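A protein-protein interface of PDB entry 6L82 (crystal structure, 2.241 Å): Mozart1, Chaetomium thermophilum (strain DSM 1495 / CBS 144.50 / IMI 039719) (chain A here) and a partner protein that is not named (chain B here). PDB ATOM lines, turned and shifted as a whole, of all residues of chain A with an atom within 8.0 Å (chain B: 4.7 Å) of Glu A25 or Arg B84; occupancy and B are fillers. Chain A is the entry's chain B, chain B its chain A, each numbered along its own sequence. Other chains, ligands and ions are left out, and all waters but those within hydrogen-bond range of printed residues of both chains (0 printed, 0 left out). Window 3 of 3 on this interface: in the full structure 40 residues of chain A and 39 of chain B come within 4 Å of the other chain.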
ATOM      1  N   GLN A  17      -0.829 -31.616 -14.587  1.00  0.00           N
ATOM      2  CA  GLN A  17      -0.104 -30.949 -15.665  1.00  0.00           C
ATOM      3  C   GLN A  17      -0.232 -29.439 -15.569  1.00  0.00           C
ATOM      4  O   GLN A  17       0.709 -28.716 -15.919  1.00  0.00           O
ATOM      5  CB  GLN A  17      -0.601 -31.432 -17.032  1.00  0.00           C
ATOM      6  CG  GLN A  17      -0.052 -32.794 -17.452  1.00  0.00           C
ATOM      7  CD  GLN A  17       1.349 -32.706 -18.040  1.00  0.00           C
ATOM      8  OE1 GLN A  17       2.349 -32.828 -17.324  1.00  0.00           O
ATOM      9  NE2 GLN A  17       1.426 -32.505 -19.353  1.00  0.00           N
ATOM     10  N   GLN A  18      -1.375 -28.945 -15.087  1.00  0.00           N
ATOM     11  CA  GLN A  18      -1.556 -27.507 -14.970  1.00  0.00           C
ATOM     12  C   GLN A  18      -0.765 -26.938 -13.795  1.00  0.00           C
ATOM     13  O   GLN A  18      -0.094 -25.902 -13.931  1.00  0.00           O
ATOM     14  CB  GLN A  18      -3.037 -27.160 -14.840  1.00  0.00           C
ATOM     15  CG  GLN A  18      -3.297 -25.654 -14.773  1.00  0.00           C
ATOM     16  CD  GLN A  18      -2.696 -24.876 -15.952  1.00  0.00           C
ATOM     17  OE1 GLN A  18      -2.421 -25.434 -17.017  1.00  0.00           O
ATOM     18  NE2 GLN A  18      -2.502 -23.574 -15.758  1.00  0.00           N
ATOM     19  N   ALA A  19      -0.842 -27.593 -12.632  1.00  0.00           N
ATOM     20  CA  ALA A  19      -0.058 -27.134 -11.491  1.00  0.00           C
ATOM     21  C   ALA A  19       1.421 -27.052 -11.854  1.00  0.00           C
ATOM     22  O   ALA A  19       2.085 -26.052 -11.561  1.00  0.00           O
ATOM     23  CB  ALA A  19      -0.279 -28.055 -10.289  1.00  0.00           C
ATOM     24  N   VAL A  20       1.939 -28.063 -12.556  1.00  0.00           N
ATOM     25  CA  VAL A  20       3.332 -28.004 -12.992  1.00  0.00           C
ATOM     26  C   VAL A  20       3.545 -26.905 -14.031  1.00  0.00           C
ATOM     27  O   VAL A  20       4.611 -26.280 -14.060  1.00  0.00           O
ATOM     28  CB  VAL A  20       3.789 -29.376 -13.519  1.00  0.00           C
ATOM     29  CG1 VAL A  20       5.224 -29.292 -14.061  1.00  0.00           C
ATOM     30  CG2 VAL A  20       3.694 -30.413 -12.408  1.00  0.00           C
ATOM     31  N   ASP A  21       2.559 -26.646 -14.896  1.00  0.00           N
ATOM     32  CA  ASP A  21       2.696 -25.551 -15.859  1.00  0.00           C
ATOM     33  C   ASP A  21       2.873 -24.214 -15.156  1.00  0.00           C
ATOM     34  O   ASP A  21       3.700 -23.395 -15.567  1.00  0.00           O
ATOM     35  CB  ASP A  21       1.478 -25.479 -16.777  1.00  0.00           C
ATOM     36  CG  ASP A  21       1.490 -26.541 -17.860  1.00  0.00           C
ATOM     37  OD1 ASP A  21       2.558 -27.155 -18.107  1.00  0.00           O
ATOM     38  OD2 ASP A  21       0.415 -26.761 -18.460  1.00  0.00           O
ATOM     39  N   ILE A  22       2.102 -23.976 -14.095  1.00  0.00           N
ATOM     40  CA  ILE A  22       2.205 -22.721 -13.365  1.00  0.00           C
ATOM     41  C   ILE A  22       3.522 -22.636 -12.596  1.00  0.00           C
ATOM     42  O   ILE A  22       4.116 -21.550 -12.486  1.00  0.00           O
ATOM     43  CB  ILE A  22       0.976 -22.565 -12.451  1.00  0.00           C
ATOM     44  CG1 ILE A  22      -0.299 -22.595 -13.300  1.00  0.00           C
ATOM     45  CG2 ILE A  22       1.080 -21.290 -11.622  1.00  0.00           C
ATOM     46  CD1 ILE A  22      -1.560 -22.890 -12.518  1.00  0.00           C
ATOM     47  N   LEU A  23       4.020 -23.765 -12.069  1.00  0.00           N
ATOM     48  CA  LEU A  23       5.324 -23.718 -11.400  1.00  0.00           C
ATOM     49  C   LEU A  23       6.426 -23.348 -12.374  1.00  0.00           C
ATOM     50  O   LEU A  23       7.286 -22.520 -12.046  1.00  0.00           O
ATOM     51  CB  LEU A  23       5.641 -25.034 -10.686  1.00  0.00           C
ATOM     52  CG  LEU A  23       4.828 -25.123  -9.396  1.00  0.00           C
ATOM     53  CD1 LEU A  23       4.625 -26.536  -8.898  1.00  0.00           C
ATOM     54  CD2 LEU A  23       5.506 -24.270  -8.348  1.00  0.00           C
ATOM     55  N   HIS A  24       6.394 -23.894 -13.597  1.00  0.00           N
ATOM     56  CA  HIS A  24       7.430 -23.501 -14.552  1.00  0.00           C
ATOM     57  C   HIS A  24       7.294 -22.043 -14.998  1.00  0.00           C
ATOM     58  O   HIS A  24       8.294 -21.422 -15.364  1.00  0.00           O
ATOM     59  CB  HIS A  24       7.435 -24.407 -15.778  1.00  0.00           C
ATOM     60  CG  HIS A  24       8.584 -24.126 -16.706  1.00  0.00           C
ATOM     61  ND1 HIS A  24       8.416 -23.592 -17.965  1.00  0.00           N
ATOM     62  CD2 HIS A  24       9.920 -24.269 -16.534  1.00  0.00           C
ATOM     63  CE1 HIS A  24       9.596 -23.444 -18.541  1.00  0.00           C
ATOM     64  NE2 HIS A  24      10.527 -23.842 -17.691  1.00  0.00           N
ATOM     65  N   GLU A  25       6.080 -21.484 -15.016  1.00  0.00           N
ATOM     66  CA  GLU A  25       5.961 -20.062 -15.331  1.00  0.00           C
ATOM     67  C   GLU A  25       6.636 -19.231 -14.255  1.00  0.00           C
ATOM     68  O   GLU A  25       7.422 -18.321 -14.550  1.00  0.00           O
ATOM     69  CB  GLU A  25       4.485 -19.667 -15.503  1.00  0.00           C
ATOM     70  CG  GLU A  25       3.760 -20.500 -16.552  1.00  0.00           C
ATOM     71  CD  GLU A  25       2.274 -20.137 -16.716  1.00  0.00           C
ATOM     72  OE1 GLU A  25       1.864 -19.053 -16.251  1.00  0.00           O
ATOM     73  OE2 GLU A  25       1.529 -20.946 -17.291  1.00  0.00           O
ATOM     74  N   ILE A  26       6.364 -19.554 -12.991  1.00  0.00           N
ATOM     75  CA  ILE A  26       7.038 -18.882 -11.883  1.00  0.00           C
ATOM     76  C   ILE A  26       8.547 -19.066 -11.990  1.00  0.00           C
ATOM     77  O   ILE A  26       9.327 -18.158 -11.663  1.00  0.00           O
ATOM     78  CB  ILE A  26       6.495 -19.410 -10.544  1.00  0.00           C
ATOM     79  CG1 ILE A  26       5.000 -19.100 -10.423  1.00  0.00           C
ATOM     80  CG2 ILE A  26       7.280 -18.831  -9.392  1.00  0.00           C
ATOM     81  CD1 ILE A  26       4.351 -19.760  -9.224  1.00  0.00           C
ATOM     82  N   ALA A  27       8.980 -20.235 -12.458  1.00  0.00           N
ATOM     83  CA  ALA A  27      10.410 -20.492 -12.604  1.00  0.00           C
ATOM     84  C   ALA A  27      11.018 -19.615 -13.683  1.00  0.00           C
ATOM     85  O   ALA A  27      12.161 -19.155 -13.545  1.00  0.00           O
ATOM     86  CB  ALA A  27      10.659 -21.973 -12.920  1.00  0.00           C
ATOM     87  N   THR A  28      10.275 -19.367 -14.770  1.00  0.00           N
ATOM     88  CA  THR A  28      10.791 -18.450 -15.788  1.00  0.00           C
ATOM     89  C   THR A  28      10.795 -17.013 -15.268  1.00  0.00           C
ATOM     90  O   THR A  28      11.744 -16.255 -15.512  1.00  0.00           O
ATOM     91  CB  THR A  28       9.957 -18.553 -17.060  1.00  0.00           C
ATOM     92  OG1 THR A  28       8.575 -18.462 -16.705  1.00  0.00           O
ATOM     93  CG2 THR A  28      10.177 -19.889 -17.751  1.00  0.00           C
ATOM     94  N   ILE A  29       9.738 -16.629 -14.540  1.00  0.00           N
ATOM     95  CA  ILE A  29       9.650 -15.292 -13.957  1.00  0.00           C
ATOM     96  C   ILE A  29      10.837 -15.032 -13.032  1.00  0.00           C
ATOM     97  O   ILE A  29      11.472 -13.978 -13.090  1.00  0.00           O
ATOM     98  CB  ILE A  29       8.310 -15.122 -13.214  1.00  0.00           C
ATOM     99  CG1 ILE A  29       7.134 -15.153 -14.191  1.00  0.00           C
ATOM    100  CG2 ILE A  29       8.278 -13.798 -12.456  1.00  0.00           C
ATOM    101  CD1 ILE A  29       5.749 -15.145 -13.481  1.00  0.00           C
ATOM    102  N   LEU A  30      11.135 -15.978 -12.150  1.00  0.00           N
ATOM    103  CA  LEU A  30      12.285 -15.862 -11.259  1.00  0.00           C
ATOM    104  C   LEU A  30      13.613 -16.099 -11.978  1.00  0.00           C
ATOM    105  O   LEU A  30      14.666 -15.994 -11.338  1.00  0.00           O
ATOM    106  CB  LEU A  30      12.124 -16.844 -10.084  1.00  0.00           C
ATOM    107  CG  LEU A  30      11.323 -16.334  -8.865  1.00  0.00           C
ATOM    108  CD1 LEU A  30      10.004 -15.679  -9.243  1.00  0.00           C
ATOM    109  CD2 LEU A  30      11.071 -17.439  -7.830  1.00  0.00           C
ATOM    110  N   ASN A  31      13.582 -16.399 -13.278  1.00  0.00           N
ATOM    111  CA  ASN A  31      14.775 -16.717 -14.064  1.00  0.00           C
ATOM    112  C   ASN A  31      15.600 -17.832 -13.421  1.00  0.00           C
ATOM    113  O   ASN A  31      16.817 -17.728 -13.269  1.00  0.00           O
ATOM    114  CB  ASN A  31      15.631 -15.472 -14.294  1.00  0.00           C
ATOM    115  CG  ASN A  31      16.621 -15.655 -15.430  1.00  0.00           C
ATOM    116  ND2 ASN A  31      17.713 -14.896 -15.377  1.00  0.00           N
ATOM    117  N   CYS A  32      14.925 -18.934 -13.077  1.00  0.00           N
ATOM    118  CA  CYS A  32      15.576 -20.048 -12.393  1.00  0.00           C
ATOM    119  C   CYS A  32      16.469 -20.882 -13.299  1.00  0.00           C
ATOM    120  O   CYS A  32      17.255 -21.679 -12.787  1.00  0.00           O
ATOM    121  CB  CYS A  32      14.524 -20.963 -11.767  1.00  0.00           C
ATOM    122  SG  CYS A  32      13.711 -20.213 -10.370  1.00  0.00           S
ATOM    123  N   LEU A  34      15.522 -23.397 -15.158  1.00  0.00           N
ATOM    124  CA  LEU A  34      15.004 -24.763 -15.173  1.00  0.00           C
ATOM    125  C   LEU A  34      14.040 -24.927 -16.334  1.00  0.00           C
ATOM    126  O   LEU A  34      13.063 -24.185 -16.426  1.00  0.00           O
ATOM    127  CB  LEU A  34      14.239 -25.063 -13.887  1.00  0.00           C
ATOM    128  CG  LEU A  34      14.947 -24.975 -12.557  1.00  0.00           C
ATOM    129  CD1 LEU A  34      13.922 -25.170 -11.484  1.00  0.00           C
ATOM    130  CD2 LEU A  34      15.992 -26.068 -12.482  1.00  0.00           C
ATOM    131  N   LEU A  39      12.478 -29.251 -13.808  1.00  0.00           N
ATOM    132  CA  LEU A  39      11.504 -29.024 -12.746  1.00  0.00           C
ATOM    133  C   LEU A  39      10.735 -30.304 -12.424  1.00  0.00           C
ATOM    134  O   LEU A  39      10.479 -30.616 -11.252  1.00  0.00           O
ATOM    135  CB  LEU A  39      10.551 -27.908 -13.163  1.00  0.00           C
ATOM    136  CG  LEU A  39       9.415 -27.606 -12.192  1.00  0.00           C
ATOM    137  CD1 LEU A  39       9.956 -27.107 -10.861  1.00  0.00           C
ATOM    138  CD2 LEU A  39       8.452 -26.606 -12.814  1.00  0.00           C
ATOM    139  N   ALA B  80       2.689 -10.572 -13.396  1.00  0.00           N
ATOM    140  CA  ALA B  80       2.850 -11.977 -13.764  1.00  0.00           C
ATOM    141  C   ALA B  80       3.013 -12.859 -12.532  1.00  0.00           C
ATOM    142  O   ALA B  80       2.267 -13.830 -12.339  1.00  0.00           O
ATOM    143  CB  ALA B  80       4.068 -12.135 -14.678  1.00  0.00           C
ATOM    144  N   LEU B  81       3.998 -12.529 -11.690  1.00  0.00           N
ATOM    145  CA  LEU B  81       4.282 -13.333 -10.503  1.00  0.00           C
ATOM    146  C   LEU B  81       3.063 -13.406  -9.611  1.00  0.00           C
ATOM    147  O   LEU B  81       2.642 -14.489  -9.198  1.00  0.00           O
ATOM    148  CB  LEU B  81       5.463 -12.743  -9.723  1.00  0.00           C
ATOM    149  CG  LEU B  81       5.913 -13.554  -8.502  1.00  0.00           C
ATOM    150  CD1 LEU B  81       6.172 -15.003  -8.890  1.00  0.00           C
ATOM    151  CD2 LEU B  81       7.161 -12.945  -7.860  1.00  0.00           C
ATOM    152  N   ARG B  82       2.478 -12.248  -9.308  1.00  0.00           N
ATOM    153  CA  ARG B  82       1.313 -12.212  -8.436  1.00  0.00           C
ATOM    154  C   ARG B  82       0.167 -13.060  -8.993  1.00  0.00           C
ATOM    155  O   ARG B  82      -0.490 -13.787  -8.238  1.00  0.00           O
ATOM    156  CB  ARG B  82       0.881 -10.756  -8.228  1.00  0.00           C
ATOM    157  CG  ARG B  82      -0.400 -10.574  -7.447  1.00  0.00           C
ATOM    158  CD  ARG B  82      -0.952  -9.148  -7.592  1.00  0.00           C
ATOM    159  NE  ARG B  82      -2.104  -9.105  -8.495  1.00  0.00           N
ATOM    160  CZ  ARG B  82      -2.163  -8.388  -9.616  1.00  0.00           C
ATOM    161  NH1 ARG B  82      -1.139  -7.624  -9.984  1.00  0.00           N
ATOM    162  NH2 ARG B  82      -3.256  -8.431 -10.366  1.00  0.00           N
ATOM    163  N   THR B  83      -0.085 -12.993 -10.310  1.00  0.00           N
ATOM    164  CA  THR B  83      -1.202 -13.752 -10.877  1.00  0.00           C
ATOM    165  C   THR B  83      -0.881 -15.234 -11.065  1.00  0.00           C
ATOM    166  O   THR B  83      -1.788 -16.066 -10.966  1.00  0.00           O
ATOM    167  CB  THR B  83      -1.660 -13.162 -12.221  1.00  0.00           C
ATOM    168  OG1 THR B  83      -0.543 -13.017 -13.102  1.00  0.00           O
ATOM    169  CG2 THR B  83      -2.353 -11.797 -12.026  1.00  0.00           C
ATOM    170  N   ARG B  84       0.366 -15.606 -11.359  1.00  0.00           N
ATOM    171  CA  ARG B  84       0.646 -17.038 -11.379  1.00  0.00           C
ATOM    172  C   ARG B  84       0.415 -17.626  -9.995  1.00  0.00           C
ATOM    173  O   ARG B  84      -0.197 -18.689  -9.869  1.00  0.00           O
ATOM    174  CB  ARG B  84       2.068 -17.366 -11.850  1.00  0.00           C
ATOM    175  CG  ARG B  84       2.686 -16.678 -13.069  1.00  0.00           C
ATOM    176  CD  ARG B  84       1.899 -16.673 -14.337  1.00  0.00           C
ATOM    177  NE  ARG B  84       0.737 -15.809 -14.304  1.00  0.00           N
ATOM    178  CZ  ARG B  84      -0.313 -16.046 -15.076  1.00  0.00           C
ATOM    179  NH1 ARG B  84      -0.289 -17.125 -15.851  1.00  0.00           N
ATOM    180  NH2 ARG B  84      -1.395 -15.260 -15.061  1.00  0.00           N
ATOM    181  N   LEU B  85       0.847 -16.924  -8.941  1.00  0.00           N
ATOM    182  CA  LEU B  85       0.601 -17.410  -7.581  1.00  0.00           C
ATOM    183  C   LEU B  85      -0.884 -17.477  -7.277  1.00  0.00           C
ATOM    184  O   LEU B  85      -1.339 -18.356  -6.535  1.00  0.00           O
ATOM    185  CB  LEU B  85       1.292 -16.525  -6.552  1.00  0.00           C
ATOM    186  CG  LEU B  85       2.803 -16.376  -6.656  1.00  0.00           C
ATOM    187  CD1 LEU B  85       3.336 -15.302  -5.726  1.00  0.00           C
ATOM    188  CD2 LEU B  85       3.428 -17.695  -6.308  1.00  0.00           C
ATOM    189  N   ASP B  86      -1.661 -16.544  -7.823  1.00  0.00           N
ATOM    190  CA  ASP B  86      -3.105 -16.689  -7.729  1.00  0.00           C
ATOM    191  C   ASP B  86      -3.571 -17.956  -8.434  1.00  0.00           C
ATOM    192  O   ASP B  86      -4.317 -18.748  -7.854  1.00  0.00           O
ATOM    193  CB  ASP B  86      -3.819 -15.450  -8.264  1.00  0.00           C
ATOM    194  CG  ASP B  86      -3.758 -14.282  -7.285  1.00  0.00           C
ATOM    195  OD1 ASP B  86      -3.497 -14.524  -6.086  1.00  0.00           O
ATOM    196  OD2 ASP B  86      -3.967 -13.127  -7.709  1.00  0.00           O
ATOM    197  N   ALA B  87      -3.113 -18.193  -9.668  1.00  0.00           N
ATOM    198  CA  ALA B  87      -3.530 -19.395 -10.383  1.00  0.00           C
ATOM    199  C   ALA B  87      -3.084 -20.669  -9.677  1.00  0.00           C
ATOM    200  O   ALA B  87      -3.677 -21.733  -9.894  1.00  0.00           O
ATOM    201  CB  ALA B  87      -2.982 -19.384 -11.811  1.00  0.00           C
ATOM    202  N   LEU B  88      -2.058 -20.587  -8.836  1.00  0.00           N
ATOM    203  CA  LEU B  88      -1.565 -21.772  -8.153  1.00  0.00           C
ATOM    204  C   LEU B  88      -2.454 -22.188  -6.979  1.00  0.00           C
ATOM    205  O   LEU B  88      -2.542 -23.388  -6.691  1.00  0.00           O
ATOM    206  CB  LEU B  88      -0.125 -21.521  -7.688  1.00  0.00           C
ATOM    207  CG  LEU B  88       0.767 -22.694  -7.285  1.00  0.00           C
ATOM    208  CD1 LEU B  88       0.882 -23.702  -8.413  1.00  0.00           C
ATOM    209  CD2 LEU B  88       2.132 -22.171  -6.917  1.00  0.00           C
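The side-chain carboxylate (OE1) of Glu A25 is in salt-bridge range of the guanidinium group (NH1) of Arg B84, at 2.9 Å.
O of Ala B80 lies within hydrogen-bond range of OG1 of Thr B83 (3.0 Å).
The guanidinium group (NE) of Arg B84 sits close to the backbone carbonyl oxygen (O) of Ala B80, at 3.2 Å.
The guanidinium group (NH2) of Arg B84 sits at hydrogen-bond distance from the side-chain hydroxyl (OG1) of Thr B83 (3.1 Å).
The side-chain hydroxyl (OG1) of Thr A28 lies within hydrogen-bond range of the backbone carbonyl oxygen (O) of Glu A25.
Among the printed residues, pairs that only touch across the chains: Ile A22 with Arg B84 (3.4 Å), Ile A22 with Ala B87 (3.6 Å), Ile A26 with Arg B84 (3.7 Å), Ile A26 with Leu B85 (3.7 Å), Ile A29 with Ala B80 (3.6 Å), Ile A29 with Leu B81 (3.6 Å), Ile A29 with Arg B84 (3.4 Å) and Leu A30 with Leu B81 (3.9 Å).
Of chain B, only Arg B84 (2.9 Å) comes within 4 Å of Glu A25.
Arg B84 touches just these residues of chain A: Ile A22, Glu A25, Ile A26 and Ile A29.
Of the printed residues of chain B, Ile A26 touches Arg B84 and Leu B85.
Of the printed residues of chain A, Ala B80 touches Ile A29.
Printed residues of chain B within 4 Å of Leu A30: Leu B81.
Of the printed residues of chain A, Ala B87 touches Ile A22.
Ala A27 touches none of the printed residues of chain B.
Ala A19 touches none of the printed residues of chain B.
The nearest printed residue of chain B that does not touch Glu A25 is Ala B80 (6.5 Å).
The nearest printed residue of chain A that does not touch Leu B85 is Ile A22 (5.1 Å).
Hydrophobic or aromatic side chains of chain B within 4 Å of the printed part of chain A: Ala B80, Leu B81, Leu B85 and Ala B87.
Along chain B the printed residues that touch a printed residue of chain A span positions 80 to 87.
Of the 18 printed residues of chain A, 5 touch a printed residue of chain B.
Among the printed residues, 9 pairs touch across the chains.
Among the printed residues, Asp or Glu carboxylates within 4 Å of a Lys or Arg side-chain nitrogen of the other chain: Glu A25 with Arg B84 (2.9 Å).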
